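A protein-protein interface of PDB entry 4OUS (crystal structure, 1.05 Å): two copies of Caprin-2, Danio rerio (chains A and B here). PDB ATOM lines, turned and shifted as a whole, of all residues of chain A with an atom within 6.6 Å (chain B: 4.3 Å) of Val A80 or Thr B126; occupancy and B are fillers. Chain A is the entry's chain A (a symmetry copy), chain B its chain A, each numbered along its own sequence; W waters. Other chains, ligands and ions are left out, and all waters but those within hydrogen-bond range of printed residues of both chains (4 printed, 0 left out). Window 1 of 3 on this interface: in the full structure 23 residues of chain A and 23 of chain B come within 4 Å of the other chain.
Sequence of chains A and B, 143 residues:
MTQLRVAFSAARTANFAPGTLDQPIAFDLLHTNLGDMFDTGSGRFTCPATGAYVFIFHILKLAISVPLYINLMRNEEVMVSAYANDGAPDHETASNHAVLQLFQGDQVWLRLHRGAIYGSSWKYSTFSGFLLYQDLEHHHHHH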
ATOM      1  N   PHE A  57     -12.626 -29.517   2.039  1.00  0.00           N
ATOM      2  CA  PHE A  57     -13.814 -29.990   2.734  1.00  0.00           C
ATOM      3  C   PHE A  57     -15.048 -29.244   2.263  1.00  0.00           C
ATOM      4  O   PHE A  57     -14.970 -28.086   1.850  1.00  0.00           O
ATOM      5  CB  PHE A  57     -13.658 -29.878   4.261  1.00  0.00           C
ATOM      6  CG  PHE A  57     -13.532 -28.472   4.782  1.00  0.00           C
ATOM      7  CD1 PHE A  57     -14.662 -27.750   5.140  1.00  0.00           C
ATOM      8  CD2 PHE A  57     -12.292 -27.886   4.960  1.00  0.00           C
ATOM      9  CE1 PHE A  57     -14.557 -26.460   5.644  1.00  0.00           C
ATOM     10  CE2 PHE A  57     -12.189 -26.595   5.466  1.00  0.00           C
ATOM     11  CZ  PHE A  57     -13.320 -25.892   5.810  1.00  0.00           C
ATOM     12  N   ILE A  70     -17.073 -23.948  10.550  1.00  0.00           N
ATOM     13  CA  ILE A  70     -16.124 -25.053  10.502  1.00  0.00           C
ATOM     14  C   ILE A  70     -14.707 -24.503  10.521  1.00  0.00           C
ATOM     15  O   ILE A  70     -14.416 -23.534   9.811  1.00  0.00           O
ATOM     16  CB  ILE A  70     -16.299 -25.894   9.213  1.00  0.00           C
ATOM     17  CG1 ILE A  70     -17.728 -26.414   9.057  1.00  0.00           C
ATOM     18  CG2 ILE A  70     -15.294 -27.031   9.160  1.00  0.00           C
ATOM     19  CD1 ILE A  70     -18.129 -27.428  10.096  1.00  0.00           C
ATOM     20  N   ASN A  71     -13.823 -25.122  11.302  1.00  0.00           N
ATOM     21  CA  ASN A  71     -12.396 -24.811  11.238  1.00  0.00           C
ATOM     22  C   ASN A  71     -11.607 -26.022  10.761  1.00  0.00           C
ATOM     23  O   ASN A  71     -11.798 -27.129  11.277  1.00  0.00           O
ATOM     24  CB  ASN A  71     -11.824 -24.400  12.601  1.00  0.00           C
ATOM     25  CG  ASN A  71     -12.661 -23.367  13.317  1.00  0.00           C
ATOM     26  OD1 ASN A  71     -13.249 -23.656  14.367  1.00  0.00           O
ATOM     27  ND2 ASN A  71     -12.701 -22.151  12.780  1.00  0.00           N
ATOM     28  N   LEU A  72     -10.687 -25.807   9.824  1.00  0.00           N
ATOM     29  CA  LEU A  72      -9.655 -26.792   9.527  1.00  0.00           C
ATOM     30  C   LEU A  72      -8.512 -26.563  10.509  1.00  0.00           C
ATOM     31  O   LEU A  72      -7.914 -25.484  10.530  1.00  0.00           O
ATOM     32  CB  LEU A  72      -9.159 -26.668   8.090  1.00  0.00           C
ATOM     33  CG  LEU A  72      -8.041 -27.637   7.691  1.00  0.00           C
ATOM     34  CD1 LEU A  72      -8.548 -29.056   7.522  1.00  0.00           C
ATOM     35  CD2 LEU A  72      -7.310 -27.157   6.430  1.00  0.00           C
ATOM     36  N   MET A  73      -8.259 -27.563  11.340  1.00  0.00           N
ATOM     37  CA  MET A  73      -7.279 -27.506  12.413  1.00  0.00           C
ATOM     38  C   MET A  73      -6.013 -28.241  12.036  1.00  0.00           C
ATOM     39  O   MET A  73      -6.072 -29.305  11.416  1.00  0.00           O
ATOM     40  CB  MET A  73      -7.844 -28.142  13.683  1.00  0.00           C
ATOM     41  CG  MET A  73      -9.216 -27.641  14.099  1.00  0.00           C
ATOM     42  SD  MET A  73      -9.223 -25.907  14.621  1.00  0.00           S
ATOM     43  CE  MET A  73      -8.191 -25.993  16.080  1.00  0.00           C
ATOM     44  N   GLU A  77      -4.371 -25.504  16.221  1.00  0.00           N
ATOM     45  CA  GLU A  77      -4.424 -24.202  15.565  1.00  0.00           C
ATOM     46  C   GLU A  77      -5.419 -24.160  14.407  1.00  0.00           C
ATOM     47  O   GLU A  77      -5.429 -25.056  13.560  1.00  0.00           O
ATOM     48  CB  GLU A  77      -3.031 -23.837  15.048  1.00  0.00           C
ATOM     49  CG  GLU A  77      -2.935 -22.465  14.416  1.00  0.00           C
ATOM     50  CD  GLU A  77      -1.539 -22.131  13.920  1.00  0.00           C
ATOM     51  OE1 GLU A  77      -0.618 -22.961  14.085  1.00  0.00           O
ATOM     52  OE2 GLU A  77      -1.364 -21.030  13.350  1.00  0.00           O
ATOM     53  N   VAL A  78      -6.223 -23.103  14.353  1.00  0.00           N
ATOM     54  CA  VAL A  78      -7.097 -22.849  13.217  1.00  0.00           C
ATOM     55  C   VAL A  78      -6.270 -22.433  12.004  1.00  0.00           C
ATOM     56  O   VAL A  78      -5.532 -21.445  12.056  1.00  0.00           O
ATOM     57  CB  VAL A  78      -8.133 -21.748  13.541  1.00  0.00           C
ATOM     58  CG1 VAL A  78      -8.913 -21.347  12.289  1.00  0.00           C
ATOM     59  CG2 VAL A  78      -9.072 -22.201  14.646  1.00  0.00           C
ATOM     60  N   MET A  79      -6.391 -23.183  10.914  1.00  0.00           N
ATOM     61  CA  MET A  79      -5.646 -22.874   9.696  1.00  0.00           C
ATOM     62  C   MET A  79      -6.494 -22.112   8.679  1.00  0.00           C
ATOM     63  O   MET A  79      -6.063 -21.070   8.179  1.00  0.00           O
ATOM     64  CB  MET A  79      -5.083 -24.151   9.082  1.00  0.00           C
ATOM     65  CG  MET A  79      -4.228 -24.965  10.066  1.00  0.00           C
ATOM     66  SD  MET A  79      -2.930 -24.068  10.973  1.00  0.00           S
ATOM     67  CE  MET A  79      -1.740 -23.812   9.660  1.00  0.00           C
ATOM     68  N   VAL A  80      -7.685 -22.624   8.362  1.00  0.00           N
ATOM     69  CA  VAL A  80      -8.672 -21.884   7.577  1.00  0.00           C
ATOM     70  C   VAL A  80     -10.043 -22.198   8.152  1.00  0.00           C
ATOM     71  O   VAL A  80     -10.201 -23.177   8.886  1.00  0.00           O
ATOM     72  CB  VAL A  80      -8.647 -22.230   6.054  1.00  0.00           C
ATOM     73  CG1 VAL A  80      -7.296 -21.923   5.427  1.00  0.00           C
ATOM     74  CG2 VAL A  80      -9.052 -23.677   5.791  1.00  0.00           C
ATOM     75  N   SER A  81     -11.032 -21.375   7.817  1.00  0.00           N
ATOM     76  CA  SER A  81     -12.378 -21.564   8.333  1.00  0.00           C
ATOM     77  C   SER A  81     -13.426 -21.402   7.245  1.00  0.00           C
ATOM     78  O   SER A  81     -13.149 -20.881   6.161  1.00  0.00           O
ATOM     79  CB  SER A  81     -12.662 -20.575   9.464  1.00  0.00           C
ATOM     80  OG  SER A  81     -11.702 -20.693  10.504  1.00  0.00           O
ATOM     81  N   ALA A  82     -14.637 -21.856   7.547  1.00  0.00           N
ATOM     82  CA  ALA A  82     -15.752 -21.715   6.626  1.00  0.00           C
ATOM     83  C   ALA A  82     -17.021 -21.409   7.398  1.00  0.00           C
ATOM     84  O   ALA A  82     -17.190 -21.838   8.536  1.00  0.00           O
ATOM     85  CB  ALA A  82     -15.929 -22.973   5.789  1.00  0.00           C
ATOM     86  N   SER A  95     -17.415 -24.551   3.069  1.00  0.00           N
ATOM     87  CA  SER A  95     -16.310 -25.217   2.393  1.00  0.00           C
ATOM     88  C   SER A  95     -15.055 -24.367   2.403  1.00  0.00           C
ATOM     89  O   SER A  95     -15.125 -23.131   2.444  1.00  0.00           O
ATOM     90  CB  SER A  95     -16.694 -25.570   0.949  1.00  0.00           C
ATOM     91  OG  SER A  95     -16.927 -24.409   0.170  1.00  0.00           O
ATOM     92  N   ASN A  96     -13.912 -25.034   2.376  1.00  0.00           N
ATOM     93  CA  ASN A  96     -12.642 -24.358   2.173  1.00  0.00           C
ATOM     94  C   ASN A  96     -11.594 -25.401   1.783  1.00  0.00           C
ATOM     95  O   ASN A  96     -11.915 -26.577   1.549  1.00  0.00           O
ATOM     96  CB  ASN A  96     -12.213 -23.553   3.409  1.00  0.00           C
ATOM     97  CG  ASN A  96     -11.473 -22.273   3.037  1.00  0.00           C
ATOM     98  OD1 ASN A  96     -10.747 -22.234   2.040  1.00  0.00           O
ATOM     99  ND2 ASN A  96     -11.641 -21.228   3.836  1.00  0.00           N
ATOM    100  N   HIS A  97     -10.351 -24.959   1.704  1.00  0.00           N
ATOM    101  CA  HIS A  97      -9.249 -25.793   1.278  1.00  0.00           C
ATOM    102  C   HIS A  97      -7.978 -25.208   1.887  1.00  0.00           C
ATOM    103  O   HIS A  97      -7.979 -24.056   2.340  1.00  0.00           O
ATOM    104  CB  HIS A  97      -9.139 -25.782  -0.241  1.00  0.00           C
ATOM    105  CG  HIS A  97      -8.553 -24.502  -0.733  1.00  0.00           C
ATOM    106  ND1 HIS A  97      -9.287 -23.345  -0.885  1.00  0.00           N
ATOM    107  CD2 HIS A  97      -7.266 -24.167  -0.976  1.00  0.00           C
ATOM    108  CE1 HIS A  97      -8.478 -22.364  -1.246  1.00  0.00           C
ATOM    109  NE2 HIS A  97      -7.246 -22.835  -1.302  1.00  0.00           N
ATOM    110  N   ALA A  98      -6.885 -25.962   1.848  1.00  0.00           N
ATOM    111  CA  ALA A  98      -5.589 -25.416   2.230  1.00  0.00           C
ATOM    112  C   ALA A  98      -4.477 -26.283   1.671  1.00  0.00           C
ATOM    113  O   ALA A  98      -4.666 -27.478   1.444  1.00  0.00           O
ATOM    114  CB  ALA A  98      -5.459 -25.317   3.746  1.00  0.00           C
ATOM    115  N   LEU A 100      -0.864 -27.177   3.155  1.00  0.00           N
ATOM    116  CA  LEU A 100      -0.148 -27.023   4.413  1.00  0.00           C
ATOM    117  C   LEU A 100       1.158 -27.783   4.428  1.00  0.00           C
ATOM    118  O   LEU A 100       1.240 -28.910   3.940  1.00  0.00           O
ATOM    119  CB  LEU A 100      -0.996 -27.515   5.582  1.00  0.00           C
ATOM    120  CG  LEU A 100      -2.373 -26.885   5.777  1.00  0.00           C
ATOM    121  CD1 LEU A 100      -3.062 -27.540   6.960  1.00  0.00           C
ATOM    122  CD2 LEU A 100      -2.272 -25.380   5.971  1.00  0.00           C
ATOM    123  N   ALA B  10      -2.826 -18.997   0.408  1.00  0.00           N
ATOM    124  CA  ALA B  10      -2.924 -17.647   0.929  1.00  0.00           C
ATOM    125  C   ALA B  10      -4.284 -17.394   1.555  1.00  0.00           C
ATOM    126  O   ALA B  10      -5.270 -18.072   1.232  1.00  0.00           O
ATOM    127  CB  ALA B  10      -2.662 -16.641  -0.174  1.00  0.00           C
ATOM    128  N   ALA B  11      -4.337 -16.401   2.435  1.00  0.00           N
ATOM    129  CA  ALA B  11      -5.588 -16.008   3.059  1.00  0.00           C
ATOM    130  C   ALA B  11      -5.601 -14.508   3.274  1.00  0.00           C
ATOM    131  O   ALA B  11      -4.546 -13.869   3.399  1.00  0.00           O
ATOM    132  CB  ALA B  11      -5.795 -16.730   4.374  1.00  0.00           C
ATOM    133  N   PHE B  27      -3.599 -10.876  -0.951  1.00  0.00           N
ATOM    134  CA  PHE B  27      -3.752 -11.812   0.160  1.00  0.00           C
ATOM    135  C   PHE B  27      -2.546 -11.666   1.067  1.00  0.00           C
ATOM    136  O   PHE B  27      -1.430 -11.966   0.654  1.00  0.00           O
ATOM    137  CB  PHE B  27      -3.874 -13.258  -0.328  1.00  0.00           C
ATOM    138  CG  PHE B  27      -5.188 -13.569  -0.989  1.00  0.00           C
ATOM    139  CD1 PHE B  27      -5.398 -13.257  -2.319  1.00  0.00           C
ATOM    140  CD2 PHE B  27      -6.209 -14.172  -0.274  1.00  0.00           C
ATOM    141  CE1 PHE B  27      -6.602 -13.535  -2.923  1.00  0.00           C
ATOM    142  CE2 PHE B  27      -7.416 -14.451  -0.869  1.00  0.00           C
ATOM    143  CZ  PHE B  27      -7.616 -14.129  -2.198  1.00  0.00           C
ATOM    144  N   HIS B  31       0.281 -19.607   4.224  1.00  0.00           N
ATOM    145  CA  HIS B  31       0.668 -20.826   4.919  1.00  0.00           C
ATOM    146  C   HIS B  31       1.837 -21.504   4.227  1.00  0.00           C
ATOM    147  O   HIS B  31       2.640 -22.175   4.879  1.00  0.00           O
ATOM    148  CB  HIS B  31      -0.502 -21.799   5.004  1.00  0.00           C
ATOM    149  CG  HIS B  31      -1.582 -21.353   5.936  1.00  0.00           C
ATOM    150  ND1 HIS B  31      -2.879 -21.140   5.524  1.00  0.00           N
ATOM    151  CD2 HIS B  31      -1.559 -21.083   7.262  1.00  0.00           C
ATOM    152  CE1 HIS B  31      -3.610 -20.755   6.555  1.00  0.00           C
ATOM    153  NE2 HIS B  31      -2.835 -20.717   7.622  1.00  0.00           N
ATOM    154  N   PHE B  57     -10.152 -21.456  -4.876  1.00  0.00           N
ATOM    155  CA  PHE B  57     -10.382 -20.291  -4.037  1.00  0.00           C
ATOM    156  C   PHE B  57     -11.741 -20.367  -3.367  1.00  0.00           C
ATOM    157  O   PHE B  57     -12.679 -20.963  -3.900  1.00  0.00           O
ATOM    158  CB  PHE B  57     -10.240 -18.982  -4.835  1.00  0.00           C
ATOM    159  CG  PHE B  57     -11.263 -18.790  -5.921  1.00  0.00           C
ATOM    160  CD1 PHE B  57     -12.464 -18.150  -5.652  1.00  0.00           C
ATOM    161  CD2 PHE B  57     -11.012 -19.202  -7.217  1.00  0.00           C
ATOM    162  CE1 PHE B  57     -13.407 -17.946  -6.652  1.00  0.00           C
ATOM    163  CE2 PHE B  57     -11.956 -18.996  -8.217  1.00  0.00           C
ATOM    164  CZ  PHE B  57     -13.144 -18.365  -7.931  1.00  0.00           C
ATOM    165  N   HIS B  58     -11.824 -19.743  -2.194  1.00  0.00           N
ATOM    166  CA  HIS B  58     -13.037 -19.642  -1.395  1.00  0.00           C
ATOM    167  C   HIS B  58     -13.071 -18.238  -0.824  1.00  0.00           C
ATOM    168  O   HIS B  58     -12.191 -17.900  -0.028  1.00  0.00           O
ATOM    169  CB  HIS B  58     -13.043 -20.658  -0.249  1.00  0.00           C
ATOM    170  CG  HIS B  58     -13.229 -22.075  -0.685  1.00  0.00           C
ATOM    171  ND1 HIS B  58     -12.194 -22.888  -1.092  1.00  0.00           N
ATOM    172  CD2 HIS B  58     -14.354 -22.820  -0.761  1.00  0.00           C
ATOM    173  CE1 HIS B  58     -12.680 -24.077  -1.406  1.00  0.00           C
ATOM    174  NE2 HIS B  58     -13.986 -24.064  -1.210  1.00  0.00           N
ATOM    175  N   ILE B  59     -14.050 -17.422  -1.207  1.00  0.00           N
ATOM    176  CA  ILE B  59     -14.071 -16.029  -0.775  1.00  0.00           C
ATOM    177  C   ILE B  59     -15.384 -15.728  -0.051  1.00  0.00           C
ATOM    178  O   ILE B  59     -16.457 -15.887  -0.625  1.00  0.00           O
ATOM    179  CB  ILE B  59     -13.895 -15.070  -1.971  1.00  0.00           C
ATOM    180  CG1 ILE B  59     -12.635 -15.411  -2.791  1.00  0.00           C
ATOM    181  CG2 ILE B  59     -13.876 -13.631  -1.496  1.00  0.00           C
ATOM    182  CD1 ILE B  59     -11.326 -15.241  -2.061  1.00  0.00           C
ATOM    183  N   TRP B 122      -9.479 -15.768  11.324  1.00  0.00           N
ATOM    184  CA  TRP B 122      -9.901 -17.159  11.141  1.00  0.00           C
ATOM    185  C   TRP B 122      -9.813 -17.615   9.678  1.00  0.00           C
ATOM    186  O   TRP B 122     -10.088 -18.774   9.382  1.00  0.00           O
ATOM    187  CB  TRP B 122     -11.302 -17.401  11.711  1.00  0.00           C
ATOM    188  CG  TRP B 122     -11.250 -17.967  13.114  1.00  0.00           C
ATOM    189  CD1 TRP B 122     -10.178 -17.958  13.961  1.00  0.00           C
ATOM    190  CD2 TRP B 122     -12.309 -18.634  13.819  1.00  0.00           C
ATOM    191  NE1 TRP B 122     -10.507 -18.567  15.153  1.00  0.00           N
ATOM    192  CE2 TRP B 122     -11.810 -18.994  15.087  1.00  0.00           C
ATOM    193  CE3 TRP B 122     -13.632 -18.959  13.500  1.00  0.00           C
ATOM    194  CZ2 TRP B 122     -12.588 -19.663  16.032  1.00  0.00           C
ATOM    195  CZ3 TRP B 122     -14.401 -19.619  14.441  1.00  0.00           C
ATOM    196  CH2 TRP B 122     -13.878 -19.967  15.688  1.00  0.00           C
ATOM    197  N   LYS B 123      -9.429 -16.706   8.784  1.00  0.00           N
ATOM    198  CA  LYS B 123      -8.993 -17.076   7.439  1.00  0.00           C
ATOM    199  C   LYS B 123     -10.081 -17.824   6.651  1.00  0.00           C
ATOM    200  O   LYS B 123      -9.912 -18.976   6.238  1.00  0.00           O
ATOM    201  CB  LYS B 123      -7.697 -17.892   7.536  1.00  0.00           C
ATOM    202  CG  LYS B 123      -6.565 -17.090   8.192  1.00  0.00           C
ATOM    203  CD  LYS B 123      -5.362 -17.948   8.573  1.00  0.00           C
ATOM    204  CE  LYS B 123      -5.501 -18.565   9.959  1.00  0.00           C
ATOM    205  NZ  LYS B 123      -5.078 -17.612  11.023  1.00  0.00           N
ATOM    206  N   TYR B 124     -11.203 -17.137   6.446  1.00  0.00           N
ATOM    207  CA  TYR B 124     -12.300 -17.643   5.622  1.00  0.00           C
ATOM    208  C   TYR B 124     -12.023 -17.516   4.126  1.00  0.00           C
ATOM    209  O   TYR B 124     -12.471 -18.349   3.334  1.00  0.00           O
ATOM    210  CB  TYR B 124     -13.592 -16.889   5.931  1.00  0.00           C
ATOM    211  CG  TYR B 124     -14.118 -17.093   7.320  1.00  0.00           C
ATOM    212  CD1 TYR B 124     -14.957 -18.156   7.608  1.00  0.00           C
ATOM    213  CD2 TYR B 124     -13.794 -16.215   8.348  1.00  0.00           C
ATOM    214  CE1 TYR B 124     -15.456 -18.351   8.879  1.00  0.00           C
ATOM    215  CE2 TYR B 124     -14.289 -16.405   9.629  1.00  0.00           C
ATOM    216  CZ  TYR B 124     -15.123 -17.474   9.877  1.00  0.00           C
ATOM    217  OH  TYR B 124     -15.634 -17.697  11.133  1.00  0.00           O
ATOM    218  N   SER B 125     -11.315 -16.458   3.743  1.00  0.00           N
ATOM    219  CA  SER B 125     -11.139 -16.088   2.346  1.00  0.00           C
ATOM    220  C   SER B 125      -9.740 -16.448   1.893  1.00  0.00           C
ATOM    221  O   SER B 125      -8.756 -15.873   2.380  1.00  0.00           O
ATOM    222  CB  SER B 125     -11.419 -14.596   2.165  1.00  0.00           C
ATOM    223  OG  SER B 125     -12.784 -14.324   2.461  1.00  0.00           O
ATOM    224  N   THR B 126      -9.661 -17.411   0.979  1.00  0.00           N
ATOM    225  CA  THR B 126      -8.435 -18.127   0.667  1.00  0.00           C
ATOM    226  C   THR B 126      -8.240 -18.307  -0.837  1.00  0.00           C
ATOM    227  O   THR B 126      -9.196 -18.303  -1.621  1.00  0.00           O
ATOM    228  CB  THR B 126      -8.459 -19.518   1.293  1.00  0.00           C
ATOM    229  OG1 THR B 126      -9.604 -20.198   0.767  1.00  0.00           O
ATOM    230  CG2 THR B 126      -8.536 -19.449   2.816  1.00  0.00           C
ATOM    231  N   PHE B 127      -6.989 -18.527  -1.218  1.00  0.00           N
ATOM    232  CA  PHE B 127      -6.591 -18.712  -2.615  1.00  0.00           C
ATOM    233  C   PHE B 127      -5.333 -19.558  -2.603  1.00  0.00           C
ATOM    234  O   PHE B 127      -4.359 -19.185  -1.950  1.00  0.00           O
ATOM    235  CB  PHE B 127      -6.345 -17.338  -3.255  1.00  0.00           C
ATOM    236  CG  PHE B 127      -5.872 -17.352  -4.703  1.00  0.00           C
ATOM    237  CD1 PHE B 127      -6.264 -18.320  -5.615  1.00  0.00           C
ATOM    238  CD2 PHE B 127      -5.050 -16.323  -5.145  1.00  0.00           C
ATOM    239  CE1 PHE B 127      -5.829 -18.255  -6.937  1.00  0.00           C
ATOM    240  CE2 PHE B 127      -4.622 -16.248  -6.451  1.00  0.00           C
ATOM    241  CZ  PHE B 127      -5.005 -17.216  -7.354  1.00  0.00           C
HETATM  242  O   HOH W   1     -14.706 -20.263   2.888  1.00  0.00           O
HETATM  243  O   HOH W   2     -16.792 -24.830  -2.586  1.00  0.00           O
HETATM  244  O   HOH W   3     -13.807 -26.854  -0.672  1.00  0.00           O
HETATM  245  O   HOH W   4      -5.134 -19.170  13.531  1.00  0.00           O
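The backbone carbonyl oxygen (O) of Met A79 sits close to a ring nitrogen (NE2) of His B31 (3.3 Å). NE2 of His B58 lies close to OG of Ser A95, 3.3 Å away. A ring nitrogen (ND1) of His B58 lies within hydrogen-bond range of a ring nitrogen (ND1) of His A97, 2.9 Å away. The side-chain hydroxyl of Ser A81 sits at hydrogen-bond distance from the backbone carbonyl oxygen of Trp B122, 2.7 Å away. O of Lys B123 lies within hydrogen-bond range of N of Ser A81 (3.1 Å). The side-chain amide nitrogen of Asn A96 is in hydrogen-bond range of the backbone carbonyl oxygen of Tyr B124 (3.0 Å). The side-chain amide oxygen of Asn A96 sits at hydrogen-bond distance from the side-chain hydroxyl of Thr B126 (2.7 Å).
N of Phe A57 is in hydrogen-bond range of O of Asn A96. N of Ala A82 lies within hydrogen-bond range of O of Ile A70 (2.8 Å). The side-chain amide nitrogen (ND2) of Asn A71 sits at hydrogen-bond distance from the side-chain hydroxyl (OG) of Ser A81 (2.9 Å). The backbone carbonyl oxygen (O) of Leu A72 is in hydrogen-bond range of the backbone NH (N) of Met A79 (2.8 Å). The backbone carbonyl oxygen of Val A80 lies within hydrogen-bond range of the backbone NH of Leu A72 (2.8 Å). O of Ser A81 sits at hydrogen-bond distance from ND2 of Asn A96, at 2.8 Å.
Among the printed residues, merely in contact across the chains: Met A79 with Lys B123 (3.1 Å), His A97 with Thr B126 (3.2 Å), Ser A81 with Tyr B124 (3.4 Å), Asn A71 with Trp B122 (3.4 Å), Val A80 with Lys B123 (3.4 Å), Asn A96 with His B58 (3.5 Å), Val A78 with Lys B123 (3.6 Å), Val A80 with Trp B122 (3.6 Å), Ala A82 with Tyr B124 (3.7 Å), Asn A96 with Lys B123 (3.7 Å), Val A80 with Thr B126 (3.8 Å), Val A78 with Trp B122 (3.9 Å) and His A97 with Phe B57 (3.96 Å).
Leu A72 touches none of the printed residues of chain B. Of the printed residues of chain B, Val A78 touches Trp B122 and Lys B123. Of the printed residues of chain B, Val A80 touches Trp B122, Lys B123 and Thr B126. Of the printed residues of chain B, His A97 touches Phe B57 (3.96 Å), His B58 (2.9 Å) and Thr B126 (3.2 Å). Ala A98 touches none of the printed residues of chain B. Printed residues of chain A within 4 Å of His B31: Met A79 (3.0 Å). Of the printed residues of chain A, His B58 touches Ser A95 (3.2 Å), Asn A96 (3.5 Å) and His A97 (2.9 Å). Of chain A, only Val A80, Asn A96 and His A97 come within 4 Å of Thr B126. The nearest printed residue of chain B that does not touch Val A80 is His B31 (4.03 Å). The nearest residue of chain A that does not touch Thr B126 is Ser A81 (5.9 Å).
Hydrophobic or aromatic side chains of chain B within 4 Å of the printed part of chain A: His B31, His B58, Trp B122 and Tyr B124. Printed residues of chain A that touch a printed residue of chain B: Asn A71, Val A78, Met A79, Val A80, Ser A81, Ala A82, Ser A95, Asn A96 and His A97.
Position printed for both chains: 57.
Water W4 bridges the backbone carbonyl oxygen of Val A78 (2.7 Å) and the side-chain amino group of Lys B123 (3.0 Å). Water W2 bridges the side-chain hydroxyl (OG) of Ser A95 (2.8 Å) and a ring nitrogen (NE2) of His B58 (3.2 Å). Water W3 lies within hydrogen-bond range of NE2 of His B58 (2.8 Å), O of Asn A96 (2.9 Å) and O of Phe A57 (3.0 Å). Water W1 lies within hydrogen-bond range of the backbone carbonyl oxygen of Ser A95 (2.9 Å), the backbone carbonyl oxygen of Tyr B124 (3.0 Å) and the side-chain amide nitrogen of Asn A96 (3.4 Å).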
